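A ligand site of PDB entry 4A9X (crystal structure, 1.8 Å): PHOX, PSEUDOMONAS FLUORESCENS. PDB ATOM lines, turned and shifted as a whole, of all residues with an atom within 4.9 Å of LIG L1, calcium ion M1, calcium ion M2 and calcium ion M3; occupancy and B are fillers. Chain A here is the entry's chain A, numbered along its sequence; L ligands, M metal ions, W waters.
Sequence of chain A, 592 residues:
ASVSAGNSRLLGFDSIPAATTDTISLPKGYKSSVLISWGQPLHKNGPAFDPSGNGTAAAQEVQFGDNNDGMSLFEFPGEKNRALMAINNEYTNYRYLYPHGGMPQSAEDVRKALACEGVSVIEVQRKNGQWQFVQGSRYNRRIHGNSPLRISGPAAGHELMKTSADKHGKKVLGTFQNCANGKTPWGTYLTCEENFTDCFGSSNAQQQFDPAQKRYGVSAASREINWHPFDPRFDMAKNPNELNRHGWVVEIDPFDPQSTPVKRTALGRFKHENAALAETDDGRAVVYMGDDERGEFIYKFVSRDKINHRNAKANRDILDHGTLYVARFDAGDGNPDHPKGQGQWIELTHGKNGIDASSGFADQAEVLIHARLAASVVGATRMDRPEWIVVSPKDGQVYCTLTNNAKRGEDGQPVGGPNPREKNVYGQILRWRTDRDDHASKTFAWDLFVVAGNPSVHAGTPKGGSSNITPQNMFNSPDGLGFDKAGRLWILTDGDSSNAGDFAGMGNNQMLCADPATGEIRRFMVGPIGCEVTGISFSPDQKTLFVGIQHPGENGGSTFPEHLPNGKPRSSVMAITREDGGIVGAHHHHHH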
ATOM      1  N   ASP A  69       8.067  29.528 -10.196  1.00  0.00           N
ATOM      2  CA  ASP A  69       9.365  30.031  -9.769  1.00  0.00           C
ATOM      3  C   ASP A  69      10.140  30.577 -10.977  1.00  0.00           C
ATOM      4  O   ASP A  69       9.664  31.520 -11.615  1.00  0.00           O
ATOM      5  CB  ASP A  69      10.034  28.890  -8.961  1.00  0.00           C
ATOM      6  CG  ASP A  69      11.103  29.249  -7.937  1.00  0.00           C
ATOM      7  OD1 ASP A  69      11.823  30.229  -8.136  1.00  0.00           O
ATOM      8  OD2 ASP A  69      11.295  28.468  -6.988  1.00  0.00           O
ATOM      9  N   GLU A  90       7.924  24.679  -8.570  1.00  0.00           N
ATOM     10  CA  GLU A  90       8.842  24.110  -7.589  1.00  0.00           C
ATOM     11  C   GLU A  90       8.270  23.100  -6.647  1.00  0.00           C
ATOM     12  O   GLU A  90       8.810  22.006  -6.503  1.00  0.00           O
ATOM     13  CB  GLU A  90       9.556  25.229  -6.797  1.00  0.00           C
ATOM     14  CG  GLU A  90      10.708  24.754  -5.922  1.00  0.00           C
ATOM     15  CD  GLU A  90      11.389  25.903  -5.200  1.00  0.00           C
ATOM     16  OE1 GLU A  90      10.663  26.767  -4.659  1.00  0.00           O
ATOM     17  OE2 GLU A  90      12.630  25.969  -5.250  1.00  0.00           O
ATOM     18  N   CYS A 179      13.454  24.816  -9.413  1.00  0.00           N
ATOM     19  CA  CYS A 179      13.671  26.095  -8.763  1.00  0.00           C
ATOM     20  C   CYS A 179      13.806  27.181  -9.838  1.00  0.00           C
ATOM     21  O   CYS A 179      12.761  27.678 -10.274  1.00  0.00           O
ATOM     22  CB  CYS A 179      14.883  25.988  -7.842  1.00  0.00           C
ATOM     23  SG  CYS A 179      15.325  27.516  -7.013  1.00  0.00           S
ATOM     24  N   GLU A 194      16.455  21.561  -7.531  1.00  0.00           N
ATOM     25  CA  GLU A 194      17.080  22.064  -6.336  1.00  0.00           C
ATOM     26  C   GLU A 194      16.925  21.128  -5.120  1.00  0.00           C
ATOM     27  O   GLU A 194      17.768  20.267  -4.955  1.00  0.00           O
ATOM     28  CB  GLU A 194      16.594  23.473  -6.056  1.00  0.00           C
ATOM     29  CG  GLU A 194      17.344  24.265  -4.963  1.00  0.00           C
ATOM     30  CD  GLU A 194      16.581  25.439  -4.366  1.00  0.00           C
ATOM     31  OE1 GLU A 194      15.342  25.439  -4.473  1.00  0.00           O
ATOM     32  OE2 GLU A 194      17.218  26.352  -3.799  1.00  0.00           O
ATOM     33  N   ASN A 195      15.865  21.273  -4.295  1.00  0.00           N
ATOM     34  CA  ASN A 195      15.685  20.440  -3.089  1.00  0.00           C
ATOM     35  C   ASN A 195      14.948  19.109  -3.351  1.00  0.00           C
ATOM     36  O   ASN A 195      14.066  18.705  -2.594  1.00  0.00           O
ATOM     37  CB  ASN A 195      15.031  21.255  -1.991  1.00  0.00           C
ATOM     38  CG  ASN A 195      15.924  22.346  -1.458  1.00  0.00           C
ATOM     39  OD1 ASN A 195      16.949  22.069  -0.838  1.00  0.00           O
ATOM     40  ND2 ASN A 195      15.552  23.608  -1.618  1.00  0.00           N
ATOM     41  N   ARG A 223      11.682  15.218   4.159  1.00  0.00           N
ATOM     42  CA  ARG A 223      11.602  16.547   4.779  1.00  0.00           C
ATOM     43  C   ARG A 223      10.149  17.024   4.707  1.00  0.00           C
ATOM     44  O   ARG A 223       9.830  18.012   4.040  1.00  0.00           O
ATOM     45  CB  ARG A 223      12.607  17.512   4.129  1.00  0.00           C
ATOM     46  CG  ARG A 223      12.875  18.765   4.945  1.00  0.00           C
ATOM     47  CD  ARG A 223      14.032  19.583   4.407  1.00  0.00           C
ATOM     48  NE  ARG A 223      15.325  18.934   4.643  1.00  0.00           N
ATOM     49  CZ  ARG A 223      16.497  19.354   4.165  1.00  0.00           C
ATOM     50  NH1 ARG A 223      16.557  20.451   3.411  1.00  0.00           N
ATOM     51  NH2 ARG A 223      17.613  18.699   4.444  1.00  0.00           N
ATOM     52  N   GLU A 273      20.072  25.828  -8.236  1.00  0.00           N
ATOM     53  CA  GLU A 273      19.175  26.962  -8.141  1.00  0.00           C
ATOM     54  C   GLU A 273      18.885  27.448  -9.588  1.00  0.00           C
ATOM     55  O   GLU A 273      17.807  27.186 -10.054  1.00  0.00           O
ATOM     56  CB  GLU A 273      19.780  28.074  -7.296  1.00  0.00           C
ATOM     57  CG  GLU A 273      18.879  29.287  -7.216  1.00  0.00           C
ATOM     58  CD  GLU A 273      17.973  29.331  -6.010  1.00  0.00           C
ATOM     59  OE1 GLU A 273      18.296  28.697  -4.982  1.00  0.00           O
ATOM     60  OE2 GLU A 273      16.975  30.078  -6.062  1.00  0.00           O
ATOM     61  N   ASP A 292      22.359  25.654  -3.785  1.00  0.00           N
ATOM     62  CA  ASP A 292      21.741  26.385  -2.677  1.00  0.00           C
ATOM     63  C   ASP A 292      21.581  25.538  -1.431  1.00  0.00           C
ATOM     64  O   ASP A 292      20.570  24.871  -1.210  1.00  0.00           O
ATOM     65  CB  ASP A 292      20.402  27.024  -3.073  1.00  0.00           C
ATOM     66  CG  ASP A 292      19.752  27.770  -1.914  1.00  0.00           C
ATOM     67  OD1 ASP A 292      20.456  28.040  -0.922  1.00  0.00           O
ATOM     68  OD2 ASP A 292      18.555  28.065  -1.996  1.00  0.00           O
ATOM     69  N   GLU A 293      22.614  25.586  -0.609  1.00  0.00           N
ATOM     70  CA  GLU A 293      22.630  24.959   0.709  1.00  0.00           C
ATOM     71  C   GLU A 293      23.762  25.625   1.486  1.00  0.00           C
ATOM     72  O   GLU A 293      24.810  25.957   0.910  1.00  0.00           O
ATOM     73  CB  GLU A 293      22.765  23.426   0.609  1.00  0.00           C
ATOM     74  CG  GLU A 293      22.909  22.713   1.945  1.00  0.00           C
ATOM     75  CD  GLU A 293      22.713  21.205   1.955  1.00  0.00           C
ATOM     76  OE1 GLU A 293      22.242  20.649   0.943  1.00  0.00           O
ATOM     77  OE2 GLU A 293      23.076  20.561   2.975  1.00  0.00           O
ATOM     78  N   ARG A 294      23.533  25.848   2.783  1.00  0.00           N
ATOM     79  CA  ARG A 294      24.530  26.473   3.669  1.00  0.00           C
ATOM     80  C   ARG A 294      25.894  25.780   3.535  1.00  0.00           C
ATOM     81  O   ARG A 294      25.983  24.580   3.678  1.00  0.00           O
ATOM     82  CB  ARG A 294      24.067  26.392   5.133  1.00  0.00           C
ATOM     83  CG  ARG A 294      22.996  27.400   5.497  1.00  0.00           C
ATOM     84  CD  ARG A 294      22.639  27.285   6.967  1.00  0.00           C
ATOM     85  NE  ARG A 294      21.864  26.064   7.264  1.00  0.00           N
ATOM     86  CZ  ARG A 294      20.535  25.961   7.255  1.00  0.00           C
ATOM     87  NH1 ARG A 294      19.781  27.018   6.959  1.00  0.00           N
ATOM     88  NH2 ARG A 294      19.952  24.805   7.545  1.00  0.00           N
ATOM     89  N   ARG A 385      24.887  30.190   0.939  1.00  0.00           N
ATOM     90  CA  ARG A 385      23.727  29.823   0.134  1.00  0.00           C
ATOM     91  C   ARG A 385      23.667  30.524  -1.223  1.00  0.00           C
ATOM     92  O   ARG A 385      22.867  31.433  -1.424  1.00  0.00           O
ATOM     93  CB  ARG A 385      22.429  30.049   0.899  1.00  0.00           C
ATOM     94  CG  ARG A 385      22.209  29.067   2.034  1.00  0.00           C
ATOM     95  CD  ARG A 385      20.834  29.192   2.620  1.00  0.00           C
ATOM     96  NE  ARG A 385      19.818  28.932   1.626  1.00  0.00           N
ATOM     97  CZ  ARG A 385      18.542  29.308   1.711  1.00  0.00           C
ATOM     98  NH1 ARG A 385      18.123  30.014   2.759  1.00  0.00           N
ATOM     99  NH2 ARG A 385      17.687  29.009   0.740  1.00  0.00           N
ATOM    100  N   GLU A 387      22.282  31.505  -4.484  1.00  0.00           N
ATOM    101  CA  GLU A 387      20.991  31.330  -5.143  1.00  0.00           C
ATOM    102  C   GLU A 387      21.121  31.755  -6.614  1.00  0.00           C
ATOM    103  O   GLU A 387      21.860  31.063  -7.307  1.00  0.00           O
ATOM    104  CB  GLU A 387      19.804  31.944  -4.365  1.00  0.00           C
ATOM    105  CG  GLU A 387      19.512  31.164  -3.084  1.00  0.00           C
ATOM    106  CD  GLU A 387      18.093  31.266  -2.537  1.00  0.00           C
ATOM    107  OE1 GLU A 387      17.273  30.350  -2.742  1.00  0.00           O
ATOM    108  OE2 GLU A 387      17.816  32.294  -1.878  1.00  0.00           O
ATOM    109  N   TRP A 388      20.452  32.819  -7.112  1.00  0.00           N
ATOM    110  CA  TRP A 388      20.539  33.093  -8.536  1.00  0.00           C
ATOM    111  C   TRP A 388      21.811  33.767  -8.966  1.00  0.00           C
ATOM    112  O   TRP A 388      22.370  34.605  -8.255  1.00  0.00           O
ATOM    113  CB  TRP A 388      19.377  33.934  -9.043  1.00  0.00           C
ATOM    114  CG  TRP A 388      18.025  33.279  -9.019  1.00  0.00           C
ATOM    115  CD1 TRP A 388      17.498  32.545  -8.013  1.00  0.00           C
ATOM    116  CD2 TRP A 388      16.944  33.552  -9.922  1.00  0.00           C
ATOM    117  NE1 TRP A 388      16.175  32.265  -8.277  1.00  0.00           N
ATOM    118  CE2 TRP A 388      15.788  32.964  -9.379  1.00  0.00           C
ATOM    119  CE3 TRP A 388      16.837  34.285 -11.107  1.00  0.00           C
ATOM    120  CZ2 TRP A 388      14.540  33.009 -10.042  1.00  0.00           C
ATOM    121  CZ3 TRP A 388      15.594  34.386 -11.727  1.00  0.00           C
ATOM    122  CH2 TRP A 388      14.486  33.691 -11.234  1.00  0.00           C
ATOM    123  N   THR A 403      21.994  34.200  -0.087  1.00  0.00           N
ATOM    124  CA  THR A 403      20.748  34.604   0.550  1.00  0.00           C
ATOM    125  C   THR A 403      20.838  34.785   2.039  1.00  0.00           C
ATOM    126  O   THR A 403      20.280  35.737   2.571  1.00  0.00           O
ATOM    127  CB  THR A 403      19.572  33.722   0.105  1.00  0.00           C
ATOM    128  OG1 THR A 403      18.375  34.471   0.213  1.00  0.00           O
ATOM    129  CG2 THR A 403      19.432  32.403   0.897  1.00  0.00           C
ATOM    130  N   ASP A 479      17.318  36.683  -3.398  1.00  0.00           N
ATOM    131  CA  ASP A 479      17.315  35.339  -3.980  1.00  0.00           C
ATOM    132  C   ASP A 479      17.379  35.437  -5.515  1.00  0.00           C
ATOM    133  O   ASP A 479      18.426  35.140  -6.098  1.00  0.00           O
ATOM    134  CB  ASP A 479      16.075  34.631  -3.419  1.00  0.00           C
ATOM    135  CG  ASP A 479      15.752  33.207  -3.848  1.00  0.00           C
ATOM    136  OD1 ASP A 479      16.281  32.772  -4.880  1.00  0.00           O
ATOM    137  OD2 ASP A 479      15.036  32.519  -3.097  1.00  0.00           O
ATOM    138  N   ASP A 494      13.354  36.685  -0.896  1.00  0.00           N
ATOM    139  CA  ASP A 494      12.713  35.529  -0.316  1.00  0.00           C
ATOM    140  C   ASP A 494      13.214  35.431   1.111  1.00  0.00           C
ATOM    141  O   ASP A 494      14.034  34.565   1.442  1.00  0.00           O
ATOM    142  CB  ASP A 494      13.056  34.270  -1.089  1.00  0.00           C
ATOM    143  CG  ASP A 494      12.617  33.029  -0.345  1.00  0.00           C
ATOM    144  OD1 ASP A 494      11.686  33.140   0.508  1.00  0.00           O
ATOM    145  OD2 ASP A 494      13.223  31.969  -0.586  1.00  0.00           O
ATOM    146  N   GLU A 532       6.738  34.886  -1.636  1.00  0.00           N
ATOM    147  CA  GLU A 532       8.080  35.290  -1.985  1.00  0.00           C
ATOM    148  C   GLU A 532       7.981  35.750  -3.452  1.00  0.00           C
ATOM    149  O   GLU A 532       7.053  35.355  -4.172  1.00  0.00           O
ATOM    150  CB  GLU A 532       9.128  34.199  -1.754  1.00  0.00           C
ATOM    151  CG  GLU A 532       9.327  33.222  -2.897  1.00  0.00           C
ATOM    152  CD  GLU A 532      10.272  32.083  -2.562  1.00  0.00           C
ATOM    153  OE1 GLU A 532       9.986  31.391  -1.562  1.00  0.00           O
ATOM    154  OE2 GLU A 532      11.315  31.941  -3.249  1.00  0.00           O
ATOM    155  N   THR A 534       9.643  35.745  -6.970  1.00  0.00           N
ATOM    156  CA  THR A 534      10.596  34.943  -7.736  1.00  0.00           C
ATOM    157  C   THR A 534      10.167  34.825  -9.165  1.00  0.00           C
ATOM    158  O   THR A 534       8.988  34.957  -9.465  1.00  0.00           O
ATOM    159  CB  THR A 534      10.772  33.596  -7.023  1.00  0.00           C
ATOM    160  OG1 THR A 534      11.789  32.835  -7.671  1.00  0.00           O
ATOM    161  CG2 THR A 534       9.453  32.831  -6.898  1.00  0.00           C
ATOM    162  N   GLN A 550       5.054  33.575  -5.503  1.00  0.00           N
ATOM    163  CA  GLN A 550       5.032  32.196  -5.093  1.00  0.00           C
ATOM    164  C   GLN A 550       4.532  32.048  -3.674  1.00  0.00           C
ATOM    165  O   GLN A 550       4.857  32.878  -2.807  1.00  0.00           O
ATOM    166  CB  GLN A 550       6.465  31.650  -5.205  1.00  0.00           C
ATOM    167  CG  GLN A 550       6.541  30.147  -5.126  1.00  0.00           C
ATOM    168  CD  GLN A 550       7.932  29.660  -4.912  1.00  0.00           C
ATOM    169  OE1 GLN A 550       8.604  30.050  -3.975  1.00  0.00           O
ATOM    170  NE2 GLN A 550       8.405  28.768  -5.772  1.00  0.00           N
ATOM    171  N   HIS A 551       3.706  31.015  -3.462  1.00  0.00           N
ATOM    172  CA  HIS A 551       3.071  30.589  -2.197  1.00  0.00           C
ATOM    173  C   HIS A 551       2.445  31.714  -1.373  1.00  0.00           C
ATOM    174  O   HIS A 551       2.683  31.857  -0.170  1.00  0.00           O
ATOM    175  CB  HIS A 551       3.982  29.693  -1.324  1.00  0.00           C
ATOM    176  CG  HIS A 551       5.290  30.309  -0.928  1.00  0.00           C
ATOM    177  ND1 HIS A 551       5.347  31.334  -0.012  1.00  0.00           N
ATOM    178  CD2 HIS A 551       6.535  30.092  -1.407  1.00  0.00           C
ATOM    179  CE1 HIS A 551       6.623  31.671   0.079  1.00  0.00           C
ATOM    180  NE2 HIS A 551       7.372  30.959  -0.744  1.00  0.00           N
HETATM  181  P1  LIG L   1      14.431  28.068  -1.536  1.00  0.00           P
HETATM  182  O1  LIG L   1      14.072  29.500  -1.755  1.00  0.00           O
HETATM  183  O2  LIG L   1      13.663  27.123  -2.490  1.00  0.00           O
HETATM  184  O3  LIG L   1      15.954  27.829  -1.676  1.00  0.00           O
HETATM  185  P2  LIG L   1      14.045  28.835   1.143  1.00  0.00           P
HETATM  186  O4  LIG L   1      15.129  29.895   0.931  1.00  0.00           O
HETATM  187  O5  LIG L   1      12.600  29.319   1.511  1.00  0.00           O
HETATM  188  C1  LIG L   1      14.065  27.557   0.054  1.00  0.00           C
HETATM  189  P3  LIG L   1      13.790  27.638   3.823  1.00  0.00           P
HETATM  190  O6  LIG L   1      12.826  26.586   3.427  1.00  0.00           O
HETATM  191  O7  LIG L   1      13.364  28.673   4.847  1.00  0.00           O
HETATM  192  O8  LIG L   1      14.509  28.410   2.607  1.00  0.00           O
HETATM  193  O9  LIG L   1      15.089  27.021   4.670  1.00  0.00           O
HETATM  194  C2  LIG L   1      16.403  27.619   4.739  1.00  0.00           C
HETATM  195  C3  LIG L   1      17.436  26.689   4.156  1.00  0.00           C
HETATM  196  O10 LIG L   1      17.572  25.523   5.002  1.00  0.00           O
HETATM  197  C4  LIG L   1      17.206  26.152   2.745  1.00  0.00           C
HETATM  198  O11 LIG L   1      18.465  25.951   2.090  1.00  0.00           O
HETATM  199  C5  LIG L   1      16.524  24.816   2.992  1.00  0.00           C
HETATM  200  O12 LIG L   1      16.746  23.902   1.927  1.00  0.00           O
HETATM  201  C6  LIG L   1      17.231  24.350   4.280  1.00  0.00           C
HETATM  202  N1  LIG L   1      16.430  23.511   5.161  1.00  0.00           N
HETATM  203  C7  LIG L   1      15.092  23.613   5.414  1.00  0.00           C
HETATM  204  N2  LIG L   1      14.639  22.745   6.292  1.00  0.00           N
HETATM  205  C8  LIG L   1      15.777  22.021   6.645  1.00  0.00           C
HETATM  206  C9  LIG L   1      15.974  20.942   7.531  1.00  0.00           C
HETATM  207  N3  LIG L   1      14.990  20.307   8.163  1.00  0.00           N
HETATM  208  N4  LIG L   1      17.230  20.461   7.656  1.00  0.00           N
HETATM  209  C10 LIG L   1      18.209  20.999   6.920  1.00  0.00           C
HETATM  210  N5  LIG L   1      18.135  22.011   6.039  1.00  0.00           N
HETATM  211  C11 LIG L   1      16.890  22.484   5.956  1.00  0.00           C
HETATM  212 FE1  LG2 L   2      14.249  27.215  -4.777  1.00  0.00          FE
HETATM  213 FE2  LG2 L   2      17.124  28.292  -3.393  1.00  0.00          FE
HETATM  214  O1  LG2 L   2      15.442  28.633  -4.230  1.00  0.00           O
HETATM  215 CA    CA M   1      15.065  30.710  -4.820  1.00  0.00          CA
HETATM  216 CA    CA M   2      15.372  31.339  -1.131  1.00  0.00          CA
HETATM  217 CA    CA M   3      11.814  30.074  -0.983  1.00  0.00          CA
HETATM  218  O   HOH W   1      16.143  33.087   0.505  1.00  0.00           O
HETATM  219  O   HOH W   2      12.837  24.619  -2.375  1.00  0.00           O
HETATM  220  O   HOH W   3      10.771  26.670   1.642  1.00  0.00           O
HETATM  221  O   HOH W   4      15.738  31.824   3.203  1.00  0.00           O
HETATM  222  O   HOH W   5      12.878  29.001  -5.124  1.00  0.00           O
HETATM  223  O   HOH W   6      14.257  30.455  -7.527  1.00  0.00           O
HETATM  224  O   HOH W   7      18.867  23.120   0.331  1.00  0.00           O
HETATM  225  O   HOH W   8      10.928  28.822  -3.018  1.00  0.00           O
HETATM  226  O   HOH W   9      20.684  25.303   3.642  1.00  0.00           O
HETATM  227  O   HOH W  10      10.657  30.861   1.062  1.00  0.00           O
HETATM  228  O   HOH W  11      12.941  32.144  -5.317  1.00  0.00           O
HETATM  229  O   HOH W  12      10.143  28.684   0.118  1.00  0.00           O
HETATM  230  O   HOH W  13      20.364  22.779   4.706  1.00  0.00           O
HETATM  231  O   HOH W  14      17.399  25.820  -0.335  1.00  0.00           O
HETATM  232  O   HOH W  15      14.597  22.048   2.221  1.00  0.00           O
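OE2 of Glu 90 lies close to O2 of LIG L1 (3.2 Å).
The side-chain carboxylate of Glu 194 lies close to an oxygen (O3) of LIG L1, 2.9 Å away.
O3 of LIG L1 lies close to OD2 of Asp 292.
The nearest printed residue that does not touch LIG L1 is Glu 273 (4.1 Å).
FE2 of LG2 L2 is bound by O3 of LIG L1.
Water W11 bridges the side-chain carboxylate (OE2) of Glu 532 (2.6 Å) and the side-chain hydroxyl (OG1) of Thr 534 (2.7 Å).
Water W5 bridges the side-chain carboxylate of Asp 69 (2.5 Å) and the side-chain carboxylate of Glu 90 (3.2 Å).
Water W6 lies within hydrogen-bond range of OD1 of Asp 69 (2.5 Å), NE1 of Trp 388 (2.7 Å) and OG1 of Thr 534 (3.4 Å).
Water W14 lies within hydrogen-bond range of O11 of LIG L1 (2.7 Å), ND2 of Asn 195 (3.2 Å), NH2 of Arg 385 (3.4 Å) and O of Asp 292 (3.4 Å).
Water W9 lies within hydrogen-bond range of an oxygen (O11) of LIG L1 (2.8 Å) and the backbone NH of Arg 294 (3.0 Å).
Water W15 lies within hydrogen-bond range of the guanidinium group of Arg 223 (2.8 Å) and an oxygen (O12) of LIG L1 (2.9 Å).
Calcium ion M3 is bound by OE1 of Glu 532 (2.3 Å).
OD2 of Asp 494 binds calcium ion M3 (2.4 Å).
Water W12 is bound to calcium ion M3, 2.4 Å away.
O1 of LIG L1 binds calcium ion M3 (2.5 Å).
Water W10 is bound to calcium ion M3, 2.5 Å away.
Water W8 binds calcium ion M3 (2.5 Å).
O5 of LIG L1 is bound to calcium ion M3, at 2.7 Å.
Calcium ion M3 has seven donor atoms within binding distance.
Slightly farther from calcium ion M3 lies OE2 of Glu 532 (3.0 Å).
Calcium ion M2 is bound by the side-chain carboxylate (OD2) of Asp 494, at 2.3 Å.
Calcium ion M2 is bound by OD2 of Asp 479 (2.3 Å).
O1 of LIG L1 is bound to calcium ion M2, at 2.3 Å.
Calcium ion M2 is bound by water W1, at 2.5 Å.
O4 of LIG L1 binds calcium ion M2, 2.5 Å away.
The side-chain carboxylate (OE1) of Glu 387 binds calcium ion M2 (2.7 Å).
Calcium ion M2 is bound by OE2 of Glu 387 (2.7 Å).
Residues that only touch calcium ion M1: Cys 179 and Trp 388.
Of the 20 residues printed, 5 come within 4 Å of calcium ion M1.
Within 4 Å of calcium ion M3: Asp 494 and Glu 532.
The nearest printed residue that does not touch calcium ion M3 is Gln 550 (4.4 Å).
Merely in contact with calcium ion M2: Arg 385.
Four residues have an atom within 4 Å of calcium ion M2: Arg 385, Glu 387, Asp 479 and Asp 494.
The nearest printed residue that does not touch calcium ion M2 is Thr 403 (4.5 Å).
O of Asp 479 lies within hydrogen-bond range of N of Trp 388, at 3.2 Å.
The side-chain carboxylate (OE1) of Glu 532 lies close to a ring nitrogen (NE2) of His 551 (2.8 Å).
The side-chain carboxylate (OE2) of Glu 273 sits close to the indole nitrogen (NE1) of Trp 388 (3.2 Å).
OD1 of Asp 292 is in salt-bridge range of NE of Arg 385, at 2.8 Å.
The guanidinium group of Arg 385 sits close to the side-chain carboxylate of Glu 387 (3.8 Å).
O of Arg 385 sits at hydrogen-bond distance from N of Thr 403, 3.2 Å away.
ND2 of Asn 195 lies close to OE1 of Glu 194 (3.4 Å).
OE1 of Glu 90 lies within hydrogen-bond range of NE2 of Gln 550, at 3.2 Å.
Calcium ion M1 is bound by an oxygen (O1) of LG2 L2 (2.2 Å), the side-chain carboxylate (OE2) of Glu 273 (2.4 Å), the side-chain carboxylate (OD1) of Asp 479 (2.4 Å), the side-chain carboxylate (OD2) of Asp 479 (2.5 Å), water W11 (2.6 Å), water W5 (2.8 Å) and water W6 (2.8 Å).
Calcium ion M1 has seven donor atoms within binding distance.
Slightly farther from calcium ion M1 lies the side-chain carboxylate (OE1) of Glu 387 (3.1 Å).
O11 of LIG L1 sits at hydrogen-bond distance from NE of Arg 385, 3.3 Å away.
N5 of LIG L1 lies close to NH1 of Arg 223, at 3.4 Å.
An oxygen (O10) of LIG L1 is in hydrogen-bond range of the guanidinium group of Arg 294 (3.3 Å).
O12 of LIG L1 sits at hydrogen-bond distance from OD1 of Asn 195 (3.3 Å).
An iron atom (FE2) of LG2 L2 is bound by the side-chain carboxylate of Glu 273 (2.0 Å).
FE2 of LG2 L2 is bound by OD2 of Asp 292 (2.0 Å).
The side-chain carboxylate of Glu 387 is bound to an iron atom (FE2) of LG2 L2 (2.2 Å).
OE2 of Glu 194 is bound to FE2 of LG2 L2, at 2.0 Å.
FE1 of LG2 L2 is bound by OE2 of Glu 90 (2.1 Å).
The side-chain sulfur (SG) of Cys 179 binds an iron atom (FE1) of LG2 L2 (2.5 Å).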
